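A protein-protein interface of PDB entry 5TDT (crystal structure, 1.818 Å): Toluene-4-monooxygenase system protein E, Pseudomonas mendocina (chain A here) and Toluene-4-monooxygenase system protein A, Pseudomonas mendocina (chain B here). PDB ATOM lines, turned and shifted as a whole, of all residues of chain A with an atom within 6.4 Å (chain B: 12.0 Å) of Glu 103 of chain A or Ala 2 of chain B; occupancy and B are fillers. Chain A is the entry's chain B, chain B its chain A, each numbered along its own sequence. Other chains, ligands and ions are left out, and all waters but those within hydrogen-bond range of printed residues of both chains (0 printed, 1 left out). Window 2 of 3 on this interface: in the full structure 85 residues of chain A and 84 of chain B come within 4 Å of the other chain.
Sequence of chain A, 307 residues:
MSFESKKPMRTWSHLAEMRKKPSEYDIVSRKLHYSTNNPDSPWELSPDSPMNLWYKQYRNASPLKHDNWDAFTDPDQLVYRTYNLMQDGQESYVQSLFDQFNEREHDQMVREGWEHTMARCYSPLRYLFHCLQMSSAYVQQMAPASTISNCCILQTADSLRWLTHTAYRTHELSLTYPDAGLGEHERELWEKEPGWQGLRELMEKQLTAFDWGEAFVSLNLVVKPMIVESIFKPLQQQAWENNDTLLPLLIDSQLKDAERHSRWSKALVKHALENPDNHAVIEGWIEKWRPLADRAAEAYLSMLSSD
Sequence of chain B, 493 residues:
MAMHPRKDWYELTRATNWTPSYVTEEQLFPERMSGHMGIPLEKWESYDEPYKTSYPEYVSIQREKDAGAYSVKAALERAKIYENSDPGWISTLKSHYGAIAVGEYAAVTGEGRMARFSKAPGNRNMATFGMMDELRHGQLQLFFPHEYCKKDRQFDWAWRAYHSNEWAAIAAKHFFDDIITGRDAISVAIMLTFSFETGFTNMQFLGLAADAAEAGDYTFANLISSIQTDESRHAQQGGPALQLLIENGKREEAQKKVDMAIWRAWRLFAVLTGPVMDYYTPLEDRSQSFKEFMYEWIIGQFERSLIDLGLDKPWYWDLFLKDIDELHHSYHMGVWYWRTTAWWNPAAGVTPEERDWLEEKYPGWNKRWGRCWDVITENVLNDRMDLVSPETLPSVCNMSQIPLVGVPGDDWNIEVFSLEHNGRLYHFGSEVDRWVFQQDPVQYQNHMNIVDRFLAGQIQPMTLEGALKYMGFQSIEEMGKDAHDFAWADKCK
Printed residues of chain B that touch a printed residue of chain A: Ala 2, Met 3, His 4 and Trp 9. Of the 11 printed residues of chain A, 5 touch a printed residue of chain B. Hydrophobic or aromatic side chains of chain A that line the printed part of chain B: Tyr 168. Among the printed residues, no Asp or Glu carboxylate lies within 4 Å of a Lys or Arg side-chain nitrogen of the other chain.
The backbone NH of Ala 2 of chain B is in hydrogen-bond range of the side-chain carboxylate of Asp 99 of chain A, 2.8 Å away. The backbone NH of Ala 2 of chain B sits at hydrogen-bond distance from the side-chain amide oxygen of Asn 102 of chain A (2.8 Å). The backbone NH of Ala 2 of chain B is in hydrogen-bond range of the side-chain carboxylate of Glu 103 of chain A, at 2.7 Å. The side-chain sulfur (SD) of Met 3 of chain B lies close to the backbone NH (N) of Asp 99 of chain A, at 3.6 Å. The side-chain sulfur (SD) of Met 3 of chain B lies close to the side-chain hydroxyl (OH) of Tyr 168 of chain A, 3.7 Å away. The backbone NH of His 4 of chain B lies within hydrogen-bond range of the side-chain hydroxyl of Tyr 168 of chain A, 2.9 Å away. A ring nitrogen (NE2) of His 4 of chain B sits at hydrogen-bond distance from the side-chain carboxylate (OE1) of Glu 172 of chain A, at 2.9 Å.
NE1 of Trp 9 of chain B is in hydrogen-bond range of O of His 4 of chain B (2.9 Å). The backbone carbonyl oxygen (O) of Pro 5 of chain B is in hydrogen-bond range of the indole nitrogen (NE1) of Trp 9 of chain B (3.2 Å). ND2 of Asn 102 of chain A lies within hydrogen-bond range of OE1 of Glu 172 of chain A, 3.1 Å away.
Among the printed residues, pairs that only touch across the chains: Tyr 168 of chain A with Trp 9 of chain B (3.4 Å) and Asn 102 of chain A with His 4 of chain B (3.6 Å).
No residue of chain B comes within 4 Å of Gln 100 of chain A. Asn 102 of chain A touches just these residues of chain B: Ala 2 and His 4. Glu 103 of chain A touches just one residue of chain B: Ala 2. Of the printed residues of chain B, Tyr 168 of chain A touches Met 3 (3.3 Å), His 4 (2.9 Å) and Trp 9 (3.4 Å). Of chain A, only Asp 99 (2.8 Å), Asn 102 (2.8 Å) and Glu 103 (2.7 Å) come within 4 Å of Ala 2 of chain B. Of the printed residues of chain A, His 4 of chain B touches Asn 102, Tyr 168 and Glu 172. Printed residues of chain A within 4 Å of Trp 9 of chain B: Tyr 168. The nearest residue of chain B that does not touch Glu 103 of chain A is Met 3 of chain B (5.9 Å).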
ATOM      1  N   PHE A  98      -4.327  11.935 -10.363  1.00  0.00           N
ATOM      2  CA  PHE A  98      -5.357  11.079 -10.940  1.00  0.00           C
ATOM      3  C   PHE A  98      -5.838  11.658 -12.262  1.00  0.00           C
ATOM      4  O   PHE A  98      -5.840  10.973 -13.287  1.00  0.00           O
ATOM      5  CB  PHE A  98      -6.547  10.913  -9.983  1.00  0.00           C
ATOM      6  CG  PHE A  98      -6.263  10.089  -8.750  1.00  0.00           C
ATOM      7  CD1 PHE A  98      -5.097   9.337  -8.622  1.00  0.00           C
ATOM      8  CD2 PHE A  98      -7.193  10.057  -7.720  1.00  0.00           C
ATOM      9  CE1 PHE A  98      -4.864   8.587  -7.476  1.00  0.00           C
ATOM     10  CE2 PHE A  98      -6.968   9.310  -6.577  1.00  0.00           C
ATOM     11  CZ  PHE A  98      -5.795   8.579  -6.455  1.00  0.00           C
ATOM     12  N   ASP A  99      -6.227  12.939 -12.251  1.00  0.00           N
ATOM     13  CA  ASP A  99      -6.703  13.628 -13.454  1.00  0.00           C
ATOM     14  C   ASP A  99      -5.706  13.516 -14.611  1.00  0.00           C
ATOM     15  O   ASP A  99      -6.063  13.068 -15.708  1.00  0.00           O
ATOM     16  CB  ASP A  99      -6.975  15.091 -13.101  1.00  0.00           C
ATOM     17  CG  ASP A  99      -7.719  15.860 -14.202  1.00  0.00           C
ATOM     18  OD1 ASP A  99      -8.300  15.248 -15.124  1.00  0.00           O
ATOM     19  OD2 ASP A  99      -7.724  17.106 -14.123  1.00  0.00           O
ATOM     20  N   GLN A 100      -4.441  13.893 -14.375  1.00  0.00           N
ATOM     21  CA  GLN A 100      -3.465  13.944 -15.467  1.00  0.00           C
ATOM     22  C   GLN A 100      -3.087  12.549 -15.958  1.00  0.00           C
ATOM     23  O   GLN A 100      -2.942  12.339 -17.172  1.00  0.00           O
ATOM     24  CB  GLN A 100      -2.203  14.701 -15.036  1.00  0.00           C
ATOM     25  CG  GLN A 100      -1.153  14.889 -16.169  1.00  0.00           C
ATOM     26  CD  GLN A 100      -1.731  15.599 -17.396  1.00  0.00           C
ATOM     27  OE1 GLN A 100      -2.467  16.576 -17.268  1.00  0.00           O
ATOM     28  NE2 GLN A 100      -1.413  15.095 -18.591  1.00  0.00           N
ATOM     29  N   PHE A 101      -2.874  11.591 -15.041  1.00  0.00           N
ATOM     30  CA  PHE A 101      -2.532  10.240 -15.488  1.00  0.00           C
ATOM     31  C   PHE A 101      -3.693   9.611 -16.249  1.00  0.00           C
ATOM     32  O   PHE A 101      -3.476   8.826 -17.179  1.00  0.00           O
ATOM     33  CB  PHE A 101      -2.119   9.365 -14.297  1.00  0.00           C
ATOM     34  CG  PHE A 101      -0.681   9.537 -13.906  1.00  0.00           C
ATOM     35  CD1 PHE A 101      -0.236  10.737 -13.362  1.00  0.00           C
ATOM     36  CD2 PHE A 101       0.236   8.512 -14.114  1.00  0.00           C
ATOM     37  CE1 PHE A 101       1.100  10.905 -13.014  1.00  0.00           C
ATOM     38  CE2 PHE A 101       1.567   8.668 -13.757  1.00  0.00           C
ATOM     39  CZ  PHE A 101       1.997   9.874 -13.209  1.00  0.00           C
ATOM     40  N   ASN A 102      -4.926   9.969 -15.892  1.00  0.00           N
ATOM     41  CA  ASN A 102      -6.077   9.483 -16.648  1.00  0.00           C
ATOM     42  C   ASN A 102      -6.105  10.078 -18.055  1.00  0.00           C
ATOM     43  O   ASN A 102      -6.444   9.378 -19.017  1.00  0.00           O
ATOM     44  CB  ASN A 102      -7.374   9.805 -15.908  1.00  0.00           C
ATOM     45  CG  ASN A 102      -8.597   9.588 -16.772  1.00  0.00           C
ATOM     46  OD1 ASN A 102      -8.976  10.453 -17.553  1.00  0.00           O
ATOM     47  ND2 ASN A 102      -9.213   8.419 -16.644  1.00  0.00           N
ATOM     48  N   GLU A 103      -5.781  11.373 -18.189  1.00  0.00           N
ATOM     49  CA  GLU A 103      -5.683  11.987 -19.514  1.00  0.00           C
ATOM     50  C   GLU A 103      -4.720  11.210 -20.399  1.00  0.00           C
ATOM     51  O   GLU A 103      -4.973  11.011 -21.594  1.00  0.00           O
ATOM     52  CB  GLU A 103      -5.209  13.444 -19.403  1.00  0.00           C
ATOM     53  CG  GLU A 103      -6.218  14.423 -18.835  1.00  0.00           C
ATOM     54  CD  GLU A 103      -7.441  14.585 -19.726  1.00  0.00           C
ATOM     55  OE1 GLU A 103      -8.531  14.151 -19.298  1.00  0.00           O
ATOM     56  OE2 GLU A 103      -7.310  15.140 -20.848  1.00  0.00           O
ATOM     57  N   ARG A 104      -3.607  10.765 -19.822  1.00  0.00           N
ATOM     58  CA  ARG A 104      -2.585  10.013 -20.532  1.00  0.00           C
ATOM     59  C   ARG A 104      -2.928   8.542 -20.721  1.00  0.00           C
ATOM     60  O   ARG A 104      -2.099   7.816 -21.276  1.00  0.00           O
ATOM     61  CB  ARG A 104      -1.262  10.099 -19.778  1.00  0.00           C
ATOM     62  CG  ARG A 104      -0.622  11.449 -19.763  1.00  0.00           C
ATOM     63  CD  ARG A 104       0.752  11.286 -19.164  1.00  0.00           C
ATOM     64  NE  ARG A 104       1.463  12.544 -19.015  1.00  0.00           N
ATOM     65  CZ  ARG A 104       2.595  12.666 -18.333  1.00  0.00           C
ATOM     66  NH1 ARG A 104       3.131  11.603 -17.743  1.00  0.00           N
ATOM     67  NH2 ARG A 104       3.195  13.847 -18.249  1.00  0.00           N
ATOM     68  N   GLU A 105      -4.085   8.078 -20.235  1.00  0.00           N
ATOM     69  CA  GLU A 105      -4.466   6.668 -20.329  1.00  0.00           C
ATOM     70  C   GLU A 105      -3.360   5.773 -19.767  1.00  0.00           C
ATOM     71  O   GLU A 105      -2.977   4.754 -20.359  1.00  0.00           O
ATOM     72  CB  GLU A 105      -4.830   6.306 -21.770  1.00  0.00           C
ATOM     73  CG  GLU A 105      -5.921   7.221 -22.323  1.00  0.00           C
ATOM     74  CD  GLU A 105      -6.061   7.149 -23.837  1.00  0.00           C
ATOM     75  OE1 GLU A 105      -7.117   7.575 -24.351  1.00  0.00           O
ATOM     76  OE2 GLU A 105      -5.124   6.676 -24.518  1.00  0.00           O
ATOM     77  N   HIS A 106      -2.834   6.191 -18.609  1.00  0.00           N
ATOM     78  CA  HIS A 106      -1.775   5.451 -17.924  1.00  0.00           C
ATOM     79  C   HIS A 106      -2.134   3.980 -17.731  1.00  0.00           C
ATOM     80  O   HIS A 106      -1.281   3.100 -17.894  1.00  0.00           O
ATOM     81  CB  HIS A 106      -1.490   6.116 -16.573  1.00  0.00           C
ATOM     82  CG  HIS A 106      -0.784   5.228 -15.592  1.00  0.00           C
ATOM     83  ND1 HIS A 106      -1.445   4.294 -14.819  1.00  0.00           N
ATOM     84  CD2 HIS A 106       0.521   5.147 -15.242  1.00  0.00           C
ATOM     85  CE1 HIS A 106      -0.574   3.664 -14.048  1.00  0.00           C
ATOM     86  NE2 HIS A 106       0.627   4.163 -14.287  1.00  0.00           N
ATOM     87  N   TYR A 168     -11.484   4.824  -5.225  1.00  0.00           N
ATOM     88  CA  TYR A 168     -11.462   5.559  -6.475  1.00  0.00           C
ATOM     89  C   TYR A 168     -10.649   4.821  -7.535  1.00  0.00           C
ATOM     90  O   TYR A 168     -11.074   4.717  -8.688  1.00  0.00           O
ATOM     91  CB  TYR A 168     -10.891   6.956  -6.243  1.00  0.00           C
ATOM     92  CG  TYR A 168     -10.932   7.822  -7.473  1.00  0.00           C
ATOM     93  CD1 TYR A 168      -9.899   7.792  -8.411  1.00  0.00           C
ATOM     94  CD2 TYR A 168     -12.013   8.659  -7.706  1.00  0.00           C
ATOM     95  CE1 TYR A 168      -9.952   8.577  -9.556  1.00  0.00           C
ATOM     96  CE2 TYR A 168     -12.064   9.459  -8.841  1.00  0.00           C
ATOM     97  CZ  TYR A 168     -11.041   9.405  -9.761  1.00  0.00           C
ATOM     98  OH  TYR A 168     -11.111  10.196 -10.886  1.00  0.00           O
ATOM     99  N   GLU A 172     -11.686   3.151 -11.081  1.00  0.00           N
ATOM    100  CA  GLU A 172     -11.028   3.674 -12.271  1.00  0.00           C
ATOM    101  C   GLU A 172     -10.357   2.558 -13.058  1.00  0.00           C
ATOM    102  O   GLU A 172     -10.521   2.466 -14.280  1.00  0.00           O
ATOM    103  CB  GLU A 172     -10.008   4.753 -11.898  1.00  0.00           C
ATOM    104  CG  GLU A 172      -9.282   5.334 -13.119  1.00  0.00           C
ATOM    105  CD  GLU A 172      -8.669   6.694 -12.858  1.00  0.00           C
ATOM    106  OE1 GLU A 172      -8.950   7.650 -13.624  1.00  0.00           O
ATOM    107  OE2 GLU A 172      -7.911   6.811 -11.877  1.00  0.00           O
ATOM    108  N   ALA B   2      -9.050  13.152 -16.875  1.00  0.00           N
ATOM    109  CA  ALA B   2     -10.400  13.456 -16.408  1.00  0.00           C
ATOM    110  C   ALA B   2     -10.625  12.815 -15.035  1.00  0.00           C
ATOM    111  O   ALA B   2      -9.840  11.936 -14.611  1.00  0.00           O
ATOM    112  CB  ALA B   2     -11.430  12.972 -17.406  1.00  0.00           C
ATOM    113  N   MET B   3     -11.671  13.269 -14.348  1.00  0.00           N
ATOM    114  CA  MET B   3     -12.068  12.770 -13.036  1.00  0.00           C
ATOM    115  C   MET B   3     -13.408  12.047 -13.128  1.00  0.00           C
ATOM    116  O   MET B   3     -14.292  12.423 -13.908  1.00  0.00           O
ATOM    117  CB  MET B   3     -12.186  13.904 -12.011  1.00  0.00           C
ATOM    118  CG  MET B   3     -10.902  14.694 -11.785  1.00  0.00           C
ATOM    119  SD  MET B   3      -9.609  13.617 -11.188  1.00  0.00           S
ATOM    120  CE  MET B   3     -10.270  13.111  -9.602  1.00  0.00           C
ATOM    121  N   HIS B   4     -13.553  10.985 -12.305  1.00  0.00           N
ATOM    122  CA  HIS B   4     -14.820  10.271 -12.310  1.00  0.00           C
ATOM    123  C   HIS B   4     -15.696  10.736 -11.148  1.00  0.00           C
ATOM    124  O   HIS B   4     -15.204  10.907 -10.028  1.00  0.00           O
ATOM    125  CB  HIS B   4     -14.565   8.766 -12.229  1.00  0.00           C
ATOM    126  CG  HIS B   4     -13.532   8.303 -13.205  1.00  0.00           C
ATOM    127  ND1 HIS B   4     -13.740   8.326 -14.567  1.00  0.00           N
ATOM    128  CD2 HIS B   4     -12.263   7.860 -13.026  1.00  0.00           C
ATOM    129  CE1 HIS B   4     -12.656   7.895 -15.186  1.00  0.00           C
ATOM    130  NE2 HIS B   4     -11.743   7.608 -14.276  1.00  0.00           N
ATOM    131  N   PRO B   5     -16.979  10.983 -11.397  1.00  0.00           N
ATOM    132  CA  PRO B   5     -17.825  11.632 -10.387  1.00  0.00           C
ATOM    133  C   PRO B   5     -18.132  10.710  -9.217  1.00  0.00           C
ATOM    134  O   PRO B   5     -18.074   9.488  -9.326  1.00  0.00           O
ATOM    135  CB  PRO B   5     -19.096  11.969 -11.168  1.00  0.00           C
ATOM    136  CG  PRO B   5     -19.166  10.901 -12.201  1.00  0.00           C
ATOM    137  CD  PRO B   5     -17.735  10.641 -12.614  1.00  0.00           C
ATOM    138  N   ARG B   6     -18.501  11.330  -8.088  1.00  0.00           N
ATOM    139  CA  ARG B   6     -18.627  10.607  -6.823  1.00  0.00           C
ATOM    140  C   ARG B   6     -19.619   9.449  -6.904  1.00  0.00           C
ATOM    141  O   ARG B   6     -19.391   8.391  -6.300  1.00  0.00           O
ATOM    142  CB  ARG B   6     -19.039  11.569  -5.700  1.00  0.00           C
ATOM    143  CG  ARG B   6     -18.898  10.945  -4.315  1.00  0.00           C
ATOM    144  CD  ARG B   6     -19.327  11.929  -3.237  1.00  0.00           C
ATOM    145  NE  ARG B   6     -20.771  12.132  -3.273  1.00  0.00           N
ATOM    146  CZ  ARG B   6     -21.399  13.179  -2.752  1.00  0.00           C
ATOM    147  NH1 ARG B   6     -20.713  14.143  -2.150  1.00  0.00           N
ATOM    148  NH2 ARG B   6     -22.720  13.256  -2.840  1.00  0.00           N
ATOM    149  N   ASP B   8     -20.149   7.284  -9.035  1.00  0.00           N
ATOM    150  CA  ASP B   8     -19.613   6.088  -9.675  1.00  0.00           C
ATOM    151  C   ASP B   8     -18.660   5.287  -8.786  1.00  0.00           C
ATOM    152  O   ASP B   8     -18.428   4.099  -9.066  1.00  0.00           O
ATOM    153  CB  ASP B   8     -18.874   6.459 -10.966  1.00  0.00           C
ATOM    154  CG  ASP B   8     -19.790   7.062 -12.028  1.00  0.00           C
ATOM    155  OD1 ASP B   8     -21.032   7.012 -11.879  1.00  0.00           O
ATOM    156  OD2 ASP B   8     -19.253   7.579 -13.022  1.00  0.00           O
ATOM    157  N   TRP B   9     -18.079   5.894  -7.747  1.00  0.00           N
ATOM    158  CA  TRP B   9     -17.189   5.161  -6.859  1.00  0.00           C
ATOM    159  C   TRP B   9     -17.617   5.229  -5.401  1.00  0.00           C
ATOM    160  O   TRP B   9     -16.980   4.581  -4.561  1.00  0.00           O
ATOM    161  CB  TRP B   9     -15.736   5.662  -7.007  1.00  0.00           C
ATOM    162  CG  TRP B   9     -15.586   7.168  -6.991  1.00  0.00           C
ATOM    163  CD1 TRP B   9     -15.528   7.999  -8.076  1.00  0.00           C
ATOM    164  CD2 TRP B   9     -15.481   8.012  -5.836  1.00  0.00           C
ATOM    165  NE1 TRP B   9     -15.401   9.304  -7.668  1.00  0.00           N
ATOM    166  CE2 TRP B   9     -15.370   9.341  -6.299  1.00  0.00           C
ATOM    167  CE3 TRP B   9     -15.476   7.771  -4.450  1.00  0.00           C
ATOM    168  CZ2 TRP B   9     -15.261  10.430  -5.434  1.00  0.00           C
ATOM    169  CZ3 TRP B   9     -15.361   8.856  -3.589  1.00  0.00           C
ATOM    170  CH2 TRP B   9     -15.258  10.172  -4.089  1.00  0.00           C
